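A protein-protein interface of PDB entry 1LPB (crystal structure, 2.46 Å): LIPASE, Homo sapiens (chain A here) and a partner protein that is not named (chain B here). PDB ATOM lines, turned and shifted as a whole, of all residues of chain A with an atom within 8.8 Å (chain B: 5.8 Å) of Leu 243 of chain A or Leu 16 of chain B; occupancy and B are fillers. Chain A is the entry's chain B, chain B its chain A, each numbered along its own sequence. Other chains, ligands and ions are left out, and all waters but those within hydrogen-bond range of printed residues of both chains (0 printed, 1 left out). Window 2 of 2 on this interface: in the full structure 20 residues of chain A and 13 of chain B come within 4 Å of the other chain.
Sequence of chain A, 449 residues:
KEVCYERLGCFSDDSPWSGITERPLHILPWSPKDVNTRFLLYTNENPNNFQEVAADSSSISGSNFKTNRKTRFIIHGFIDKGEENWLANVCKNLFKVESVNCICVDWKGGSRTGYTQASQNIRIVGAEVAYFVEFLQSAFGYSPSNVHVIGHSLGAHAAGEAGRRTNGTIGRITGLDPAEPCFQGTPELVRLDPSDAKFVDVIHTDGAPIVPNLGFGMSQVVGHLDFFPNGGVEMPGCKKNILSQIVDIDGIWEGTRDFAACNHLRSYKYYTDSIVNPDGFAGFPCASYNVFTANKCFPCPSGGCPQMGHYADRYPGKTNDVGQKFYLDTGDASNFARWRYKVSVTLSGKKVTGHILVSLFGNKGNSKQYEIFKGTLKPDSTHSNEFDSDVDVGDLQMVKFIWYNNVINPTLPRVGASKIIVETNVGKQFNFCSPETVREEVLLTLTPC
N of Leu 16 of chain B sits at hydrogen-bond distance from OG of Ser 244 of chain A, at 3.3 Å.
The guanidinium group (NH1) of Arg 38 of chain B is in hydrogen-bond range of the backbone carbonyl oxygen (O) of Val 247 of chain A (2.4 Å).
N of Asn 241 of chain A lies within hydrogen-bond range of OE2 of Glu 15 of chain B, at 2.8 Å.
The side-chain carboxylate (OE1) of Glu 15 of chain B sits at hydrogen-bond distance from the backbone NH (N) of Asp 12 of chain B, at 2.9 Å.
The side-chain amino group of Lys 240 of chain A is in salt-bridge range of the side-chain carboxylate of Asp 248 of chain A (3.98 Å).
O of Glu 15 of chain B sits at hydrogen-bond distance from N of Cys 39 of chain B (2.8 Å).
OG of Ser 244 of chain A sits at hydrogen-bond distance from OD1 of Asn 241 of chain A (2.6 Å).
SG of Cys 17 of chain B forms a disulfide with SG of Cys 28 of chain B, 2.0 Å away.
Among the printed residues, pairs that only touch across the chains: Lys 240 of chain A with Glu 15 of chain B (3.1 Å), Ser 244 of chain A with Glu 15 of chain B (3.3 Å), Val 247 of chain A with Leu 36 of chain B (3.5 Å), Ile 249 of chain A with Arg 38 of chain B (3.6 Å), Asp 248 of chain A with Arg 38 of chain B (3.7 Å) and Leu 243 of chain A with Leu 16 of chain B (3.7 Å).
Of the printed residues of chain B, Leu 243 of chain A touches Leu 16 (3.7 Å).
Leu 16 of chain B touches two residues of chain A.
No residue of chain A comes within 4 Å of Cys 17 of chain B.
Of the printed residues of chain B, Lys 240 of chain A touches Glu 15 (3.1 Å).
Of the printed residues of chain A, Arg 38 of chain B touches Val 247, Asp 248 and Ile 249.
Of the printed residues of chain B, Ile 249 of chain A touches Arg 38 (3.6 Å).
Ile 252 of chain A touches none of the printed residues of chain B.
Gly 14 of chain B touches none of the printed residues of chain A.
Printed residues of chain A that touch a printed residue of chain B: Lys 240, Asn 241, Leu 243, Ser 244, Val 247, Asp 248 and Ile 249.
Among the printed residues, 9 pairs touch across the chains.
Among the printed residues, no Asp or Glu carboxylate lies within 4 Å of a Lys or Arg side-chain nitrogen of the other chain.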
ATOM      1  N   LYS A 240     -22.343 -24.388 -13.332  1.00  0.00           N
ATOM      2  CA  LYS A 240     -23.186 -24.377 -14.522  1.00  0.00           C
ATOM      3  C   LYS A 240     -24.428 -25.211 -14.154  1.00  0.00           C
ATOM      4  O   LYS A 240     -24.415 -25.942 -13.161  1.00  0.00           O
ATOM      5  CB  LYS A 240     -22.471 -25.046 -15.709  1.00  0.00           C
ATOM      6  CG  LYS A 240     -21.158 -24.451 -16.180  1.00  0.00           C
ATOM      7  CD  LYS A 240     -20.545 -25.429 -17.183  1.00  0.00           C
ATOM      8  CE  LYS A 240     -19.349 -24.864 -17.939  1.00  0.00           C
ATOM      9  NZ  LYS A 240     -18.104 -24.801 -17.123  1.00  0.00           N
ATOM     10  N   ASN A 241     -25.490 -25.127 -14.948  1.00  0.00           N
ATOM     11  CA  ASN A 241     -26.671 -25.917 -14.644  1.00  0.00           C
ATOM     12  C   ASN A 241     -26.372 -27.371 -14.966  1.00  0.00           C
ATOM     13  O   ASN A 241     -25.494 -27.673 -15.772  1.00  0.00           O
ATOM     14  CB  ASN A 241     -27.949 -25.411 -15.343  1.00  0.00           C
ATOM     15  CG  ASN A 241     -27.789 -25.259 -16.834  1.00  0.00           C
ATOM     16  OD1 ASN A 241     -27.382 -26.186 -17.529  1.00  0.00           O
ATOM     17  ND2 ASN A 241     -28.111 -24.080 -17.337  1.00  0.00           N
ATOM     18  N   ILE A 242     -27.125 -28.252 -14.321  1.00  0.00           N
ATOM     19  CA  ILE A 242     -26.966 -29.693 -14.399  1.00  0.00           C
ATOM     20  C   ILE A 242     -26.751 -30.324 -15.774  1.00  0.00           C
ATOM     21  O   ILE A 242     -25.844 -31.136 -15.955  1.00  0.00           O
ATOM     22  CB  ILE A 242     -28.120 -30.366 -13.603  1.00  0.00           C
ATOM     23  CG1 ILE A 242     -27.834 -31.850 -13.308  1.00  0.00           C
ATOM     24  CG2 ILE A 242     -29.431 -30.133 -14.304  1.00  0.00           C
ATOM     25  CD1 ILE A 242     -28.148 -32.814 -14.422  1.00  0.00           C
ATOM     26  N   LEU A 243     -27.540 -29.911 -16.751  1.00  0.00           N
ATOM     27  CA  LEU A 243     -27.446 -30.471 -18.090  1.00  0.00           C
ATOM     28  C   LEU A 243     -26.126 -30.109 -18.793  1.00  0.00           C
ATOM     29  O   LEU A 243     -25.570 -30.911 -19.548  1.00  0.00           O
ATOM     30  CB  LEU A 243     -28.654 -30.003 -18.910  1.00  0.00           C
ATOM     31  CG  LEU A 243     -29.469 -30.996 -19.750  1.00  0.00           C
ATOM     32  CD1 LEU A 243     -29.560 -30.458 -21.157  1.00  0.00           C
ATOM     33  CD2 LEU A 243     -28.850 -32.379 -19.745  1.00  0.00           C
ATOM     34  N   SER A 244     -25.627 -28.907 -18.497  1.00  0.00           N
ATOM     35  CA  SER A 244     -24.391 -28.364 -19.066  1.00  0.00           C
ATOM     36  C   SER A 244     -23.143 -28.951 -18.419  1.00  0.00           C
ATOM     37  O   SER A 244     -22.146 -29.150 -19.095  1.00  0.00           O
ATOM     38  CB  SER A 244     -24.379 -26.840 -18.922  1.00  0.00           C
ATOM     39  OG  SER A 244     -25.578 -26.253 -19.411  1.00  0.00           O
ATOM     40  N   GLN A 245     -23.179 -29.209 -17.111  1.00  0.00           N
ATOM     41  CA  GLN A 245     -22.029 -29.806 -16.423  1.00  0.00           C
ATOM     42  C   GLN A 245     -21.798 -31.194 -16.988  1.00  0.00           C
ATOM     43  O   GLN A 245     -20.685 -31.539 -17.393  1.00  0.00           O
ATOM     44  CB  GLN A 245     -22.270 -29.954 -14.917  1.00  0.00           C
ATOM     45  CG  GLN A 245     -22.374 -28.658 -14.120  1.00  0.00           C
ATOM     46  CD  GLN A 245     -21.035 -28.184 -13.558  1.00  0.00           C
ATOM     47  OE1 GLN A 245     -20.191 -27.665 -14.284  1.00  0.00           O
ATOM     48  NE2 GLN A 245     -20.853 -28.339 -12.253  1.00  0.00           N
ATOM     49  N   ILE A 246     -22.879 -31.967 -17.053  1.00  0.00           N
ATOM     50  CA  ILE A 246     -22.842 -33.345 -17.537  1.00  0.00           C
ATOM     51  C   ILE A 246     -22.497 -33.509 -19.023  1.00  0.00           C
ATOM     52  O   ILE A 246     -21.714 -34.403 -19.394  1.00  0.00           O
ATOM     53  CB  ILE A 246     -24.151 -34.072 -17.131  1.00  0.00           C
ATOM     54  CG1 ILE A 246     -24.117 -34.311 -15.620  1.00  0.00           C
ATOM     55  CG2 ILE A 246     -24.318 -35.384 -17.873  1.00  0.00           C
ATOM     56  CD1 ILE A 246     -25.373 -34.816 -15.038  1.00  0.00           C
ATOM     57  N   VAL A 247     -23.051 -32.617 -19.853  1.00  0.00           N
ATOM     58  CA  VAL A 247     -22.819 -32.605 -21.306  1.00  0.00           C
ATOM     59  C   VAL A 247     -21.769 -31.529 -21.634  1.00  0.00           C
ATOM     60  O   VAL A 247     -22.023 -30.602 -22.411  1.00  0.00           O
ATOM     61  CB  VAL A 247     -24.145 -32.282 -22.087  1.00  0.00           C
ATOM     62  CG1 VAL A 247     -23.992 -32.613 -23.584  1.00  0.00           C
ATOM     63  CG2 VAL A 247     -25.337 -33.032 -21.458  1.00  0.00           C
ATOM     64  N   ASP A 248     -20.608 -31.610 -20.997  1.00  0.00           N
ATOM     65  CA  ASP A 248     -19.574 -30.622 -21.257  1.00  0.00           C
ATOM     66  C   ASP A 248     -18.636 -31.134 -22.348  1.00  0.00           C
ATOM     67  O   ASP A 248     -18.597 -32.329 -22.651  1.00  0.00           O
ATOM     68  CB  ASP A 248     -18.815 -30.277 -19.969  1.00  0.00           C
ATOM     69  CG  ASP A 248     -18.443 -28.798 -19.880  1.00  0.00           C
ATOM     70  OD1 ASP A 248     -17.418 -28.406 -20.478  1.00  0.00           O
ATOM     71  OD2 ASP A 248     -19.165 -28.027 -19.201  1.00  0.00           O
ATOM     72  N   ILE A 249     -17.891 -30.203 -22.933  1.00  0.00           N
ATOM     73  CA  ILE A 249     -16.941 -30.445 -24.023  1.00  0.00           C
ATOM     74  C   ILE A 249     -16.010 -31.667 -23.981  1.00  0.00           C
ATOM     75  O   ILE A 249     -15.435 -32.017 -25.011  1.00  0.00           O
ATOM     76  CB  ILE A 249     -16.093 -29.182 -24.255  1.00  0.00           C
ATOM     77  CG1 ILE A 249     -15.249 -28.878 -23.003  1.00  0.00           C
ATOM     78  CG2 ILE A 249     -17.018 -28.000 -24.586  1.00  0.00           C
ATOM     79  CD1 ILE A 249     -14.594 -27.505 -22.964  1.00  0.00           C
ATOM     80  N   ILE A 252     -19.348 -37.299 -21.459  1.00  0.00           N
ATOM     81  CA  ILE A 252     -20.190 -37.580 -20.301  1.00  0.00           C
ATOM     82  C   ILE A 252     -19.386 -37.854 -19.034  1.00  0.00           C
ATOM     83  O   ILE A 252     -19.548 -37.135 -18.055  1.00  0.00           O
ATOM     84  CB  ILE A 252     -21.180 -38.765 -20.608  1.00  0.00           C
ATOM     85  CG1 ILE A 252     -22.273 -38.299 -21.573  1.00  0.00           C
ATOM     86  CG2 ILE A 252     -21.837 -39.304 -19.334  1.00  0.00           C
ATOM     87  CD1 ILE A 252     -21.796 -38.046 -22.972  1.00  0.00           C
ATOM     88  N   GLY A 255     -17.923 -34.906 -17.509  1.00  0.00           N
ATOM     89  CA  GLY A 255     -19.067 -34.110 -17.077  1.00  0.00           C
ATOM     90  C   GLY A 255     -19.690 -34.595 -15.779  1.00  0.00           C
ATOM     91  O   GLY A 255     -19.969 -33.815 -14.862  1.00  0.00           O
ATOM     92  N   THR A 256     -19.884 -35.899 -15.692  1.00  0.00           N
ATOM     93  CA  THR A 256     -20.457 -36.544 -14.521  1.00  0.00           C
ATOM     94  C   THR A 256     -19.576 -36.367 -13.271  1.00  0.00           C
ATOM     95  O   THR A 256     -20.061 -36.046 -12.178  1.00  0.00           O
ATOM     96  CB  THR A 256     -20.661 -38.021 -14.852  1.00  0.00           C
ATOM     97  OG1 THR A 256     -21.583 -38.116 -15.957  1.00  0.00           O
ATOM     98  CG2 THR A 256     -21.162 -38.792 -13.646  1.00  0.00           C
ATOM     99  N   PHE A 259     -20.065 -32.995 -12.235  1.00  0.00           N
ATOM    100  CA  PHE A 259     -21.353 -32.748 -11.607  1.00  0.00           C
ATOM    101  C   PHE A 259     -21.187 -33.091 -10.128  1.00  0.00           C
ATOM    102  O   PHE A 259     -21.644 -32.375  -9.246  1.00  0.00           O
ATOM    103  CB  PHE A 259     -22.455 -33.617 -12.217  1.00  0.00           C
ATOM    104  CG  PHE A 259     -23.761 -33.534 -11.471  1.00  0.00           C
ATOM    105  CD1 PHE A 259     -24.514 -32.365 -11.486  1.00  0.00           C
ATOM    106  CD2 PHE A 259     -24.192 -34.590 -10.681  1.00  0.00           C
ATOM    107  CE1 PHE A 259     -25.659 -32.254 -10.722  1.00  0.00           C
ATOM    108  CE2 PHE A 259     -25.341 -34.484  -9.912  1.00  0.00           C
ATOM    109  CZ  PHE A 259     -26.071 -33.314  -9.932  1.00  0.00           C
ATOM    110  N   GLY B   6     -32.261 -24.541 -22.360  1.00  0.00           N
ATOM    111  CA  GLY B   6     -33.589 -24.263 -23.004  1.00  0.00           C
ATOM    112  C   GLY B   6     -34.395 -23.502 -21.982  1.00  0.00           C
ATOM    113  O   GLY B   6     -34.227 -23.782 -20.802  1.00  0.00           O
ATOM    114  N   ILE B   8     -34.323 -20.637 -20.255  1.00  0.00           N
ATOM    115  CA  ILE B   8     -33.496 -20.238 -19.135  1.00  0.00           C
ATOM    116  C   ILE B   8     -32.588 -19.179 -19.764  1.00  0.00           C
ATOM    117  O   ILE B   8     -31.951 -19.397 -20.806  1.00  0.00           O
ATOM    118  CB  ILE B   8     -32.764 -21.454 -18.476  1.00  0.00           C
ATOM    119  CG1 ILE B   8     -31.941 -21.005 -17.263  1.00  0.00           C
ATOM    120  CG2 ILE B   8     -31.956 -22.231 -19.499  1.00  0.00           C
ATOM    121  CD1 ILE B   8     -31.480 -22.151 -16.369  1.00  0.00           C
ATOM    122  N   LEU B  11     -27.687 -16.988 -19.252  1.00  0.00           N
ATOM    123  CA  LEU B  11     -26.726 -18.069 -19.218  1.00  0.00           C
ATOM    124  C   LEU B  11     -25.278 -17.586 -19.323  1.00  0.00           C
ATOM    125  O   LEU B  11     -24.985 -16.549 -19.940  1.00  0.00           O
ATOM    126  CB  LEU B  11     -27.012 -19.030 -20.378  1.00  0.00           C
ATOM    127  CG  LEU B  11     -27.884 -20.271 -20.160  1.00  0.00           C
ATOM    128  CD1 LEU B  11     -29.042 -20.000 -19.226  1.00  0.00           C
ATOM    129  CD2 LEU B  11     -28.355 -20.784 -21.498  1.00  0.00           C
ATOM    130  N   ASP B  12     -24.381 -18.397 -18.768  1.00  0.00           N
ATOM    131  CA  ASP B  12     -22.948 -18.140 -18.774  1.00  0.00           C
ATOM    132  C   ASP B  12     -22.273 -18.866 -19.918  1.00  0.00           C
ATOM    133  O   ASP B  12     -22.826 -19.812 -20.506  1.00  0.00           O
ATOM    134  CB  ASP B  12     -22.313 -18.611 -17.476  1.00  0.00           C
ATOM    135  CG  ASP B  12     -22.859 -17.895 -16.280  1.00  0.00           C
ATOM    136  OD1 ASP B  12     -22.833 -16.638 -16.265  1.00  0.00           O
ATOM    137  OD2 ASP B  12     -23.333 -18.599 -15.364  1.00  0.00           O
ATOM    138  N   GLY B  14     -20.165 -21.369 -21.997  1.00  0.00           N
ATOM    139  CA  GLY B  14     -20.027 -22.794 -21.791  1.00  0.00           C
ATOM    140  C   GLY B  14     -21.332 -23.488 -21.446  1.00  0.00           C
ATOM    141  O   GLY B  14     -21.399 -24.726 -21.447  1.00  0.00           O
ATOM    142  N   GLU B  15     -22.355 -22.713 -21.096  1.00  0.00           N
ATOM    143  CA  GLU B  15     -23.659 -23.285 -20.788  1.00  0.00           C
ATOM    144  C   GLU B  15     -24.362 -23.531 -22.120  1.00  0.00           C
ATOM    145  O   GLU B  15     -24.211 -22.739 -23.052  1.00  0.00           O
ATOM    146  CB  GLU B  15     -24.456 -22.314 -19.945  1.00  0.00           C
ATOM    147  CG  GLU B  15     -25.215 -22.995 -18.853  1.00  0.00           C
ATOM    148  CD  GLU B  15     -25.177 -22.215 -17.559  1.00  0.00           C
ATOM    149  OE1 GLU B  15     -25.225 -20.969 -17.596  1.00  0.00           O
ATOM    150  OE2 GLU B  15     -25.098 -22.846 -16.494  1.00  0.00           O
ATOM    151  N   LEU B  16     -25.052 -24.658 -22.255  1.00  0.00           N
ATOM    152  CA  LEU B  16     -25.757 -24.967 -23.512  1.00  0.00           C
ATOM    153  C   LEU B  16     -26.861 -23.944 -23.803  1.00  0.00           C
ATOM    154  O   LEU B  16     -27.478 -23.378 -22.883  1.00  0.00           O
ATOM    155  CB  LEU B  16     -26.392 -26.353 -23.465  1.00  0.00           C
ATOM    156  CG  LEU B  16     -25.513 -27.586 -23.372  1.00  0.00           C
ATOM    157  CD1 LEU B  16     -26.148 -28.548 -22.398  1.00  0.00           C
ATOM    158  CD2 LEU B  16     -25.322 -28.215 -24.729  1.00  0.00           C
ATOM    159  N   CYS B  17     -27.137 -23.732 -25.079  1.00  0.00           N
ATOM    160  CA  CYS B  17     -28.167 -22.798 -25.447  1.00  0.00           C
ATOM    161  C   CYS B  17     -28.766 -23.228 -26.758  1.00  0.00           C
ATOM    162  O   CYS B  17     -28.188 -24.019 -27.498  1.00  0.00           O
ATOM    163  CB  CYS B  17     -27.598 -21.387 -25.562  1.00  0.00           C
ATOM    164  SG  CYS B  17     -26.030 -21.364 -26.456  1.00  0.00           S
ATOM    165  N   LEU B  18     -29.946 -22.686 -27.017  1.00  0.00           N
ATOM    166  CA  LEU B  18     -30.710 -22.944 -28.213  1.00  0.00           C
ATOM    167  C   LEU B  18     -30.701 -21.682 -29.047  1.00  0.00           C
ATOM    168  O   LEU B  18     -30.785 -21.747 -30.271  1.00  0.00           O
ATOM    169  CB  LEU B  18     -32.152 -23.304 -27.829  1.00  0.00           C
ATOM    170  CG  LEU B  18     -32.464 -24.770 -27.498  1.00  0.00           C
ATOM    171  CD1 LEU B  18     -32.189 -25.638 -28.704  1.00  0.00           C
ATOM    172  CD2 LEU B  18     -31.655 -25.269 -26.324  1.00  0.00           C
ATOM    173  N   GLN B  22     -30.565 -16.232 -24.985  1.00  0.00           N
ATOM    174  CA  GLN B  22     -30.312 -16.816 -23.664  1.00  0.00           C
ATOM    175  C   GLN B  22     -28.937 -16.489 -23.040  1.00  0.00           C
ATOM    176  O   GLN B  22     -28.773 -16.538 -21.807  1.00  0.00           O
ATOM    177  CB  GLN B  22     -30.431 -18.332 -23.718  1.00  0.00           C
ATOM    178  CG  GLN B  22     -31.545 -18.868 -24.568  1.00  0.00           C
ATOM    179  CD  GLN B  22     -31.588 -20.390 -24.545  1.00  0.00           C
ATOM    180  OE1 GLN B  22     -31.561 -21.047 -25.589  1.00  0.00           O
ATOM    181  NE2 GLN B  22     -31.643 -20.958 -23.337  1.00  0.00           N
ATOM    182  N   CYS B  28     -24.712 -17.619 -29.017  1.00  0.00           N
ATOM    183  CA  CYS B  28     -24.846 -19.036 -28.729  1.00  0.00           C
ATOM    184  C   CYS B  28     -24.019 -19.553 -29.887  1.00  0.00           C
ATOM    185  O   CYS B  28     -24.301 -19.219 -31.035  1.00  0.00           O
ATOM    186  CB  CYS B  28     -26.299 -19.516 -28.838  1.00  0.00           C
ATOM    187  SG  CYS B  28     -26.490 -21.287 -28.427  1.00  0.00           S
ATOM    188  N   LEU B  36     -23.679 -29.610 -30.436  1.00  0.00           N
ATOM    189  CA  LEU B  36     -24.324 -28.771 -29.440  1.00  0.00           C
ATOM    190  C   LEU B  36     -23.725 -27.386 -29.332  1.00  0.00           C
ATOM    191  O   LEU B  36     -22.527 -27.218 -29.470  1.00  0.00           O
ATOM    192  CB  LEU B  36     -24.255 -29.482 -28.110  1.00  0.00           C
ATOM    193  CG  LEU B  36     -25.021 -30.793 -28.156  1.00  0.00           C
ATOM    194  CD1 LEU B  36     -24.817 -31.517 -26.849  1.00  0.00           C
ATOM    195  CD2 LEU B  36     -26.509 -30.512 -28.430  1.00  0.00           C
ATOM    196  N   SER B  37     -24.553 -26.382 -29.079  1.00  0.00           N
ATOM    197  CA  SER B  37     -24.034 -25.025 -28.987  1.00  0.00           C
ATOM    198  C   SER B  37     -24.119 -24.471 -27.579  1.00  0.00           C
ATOM    199  O   SER B  37     -25.068 -24.755 -26.852  1.00  0.00           O
ATOM    200  CB  SER B  37     -24.738 -24.111 -30.000  1.00  0.00           C
ATOM    201  OG  SER B  37     -26.099 -23.888 -29.685  1.00  0.00           O
ATOM    202  N   ARG B  38     -23.096 -23.728 -27.169  1.00  0.00           N
ATOM    203  CA  ARG B  38     -23.055 -23.149 -25.832  1.00  0.00           C
ATOM    204  C   ARG B  38     -22.724 -21.667 -25.912  1.00  0.00           C
ATOM    205  O   ARG B  38     -22.322 -21.170 -26.956  1.00  0.00           O
ATOM    206  CB  ARG B  38     -22.032 -23.892 -24.967  1.00  0.00           C
ATOM    207  CG  ARG B  38     -22.148 -25.413 -25.073  1.00  0.00           C
ATOM    208  CD  ARG B  38     -21.291 -26.134 -24.059  1.00  0.00           C
ATOM    209  NE  ARG B  38     -20.800 -27.396 -24.600  1.00  0.00           N
ATOM    210  CZ  ARG B  38     -21.409 -28.568 -24.458  1.00  0.00           C
ATOM    211  NH1 ARG B  38     -22.553 -28.656 -23.794  1.00  0.00           N
ATOM    212  NH2 ARG B  38     -20.845 -29.668 -24.935  1.00  0.00           N
ATOM    213  N   CYS B  39     -22.907 -20.941 -24.829  1.00  0.00           N
ATOM    214  CA  CYS B  39     -22.624 -19.527 -24.870  1.00  0.00           C
ATOM    215  C   CYS B  39     -21.137 -19.278 -24.990  1.00  0.00           C
ATOM    216  O   CYS B  39     -20.338 -19.896 -24.283  1.00  0.00           O
ATOM    217  CB  CYS B  39     -23.196 -18.847 -23.644  1.00  0.00           C
ATOM    218  SG  CYS B  39     -24.976 -19.139 -23.468  1.00  0.00           S
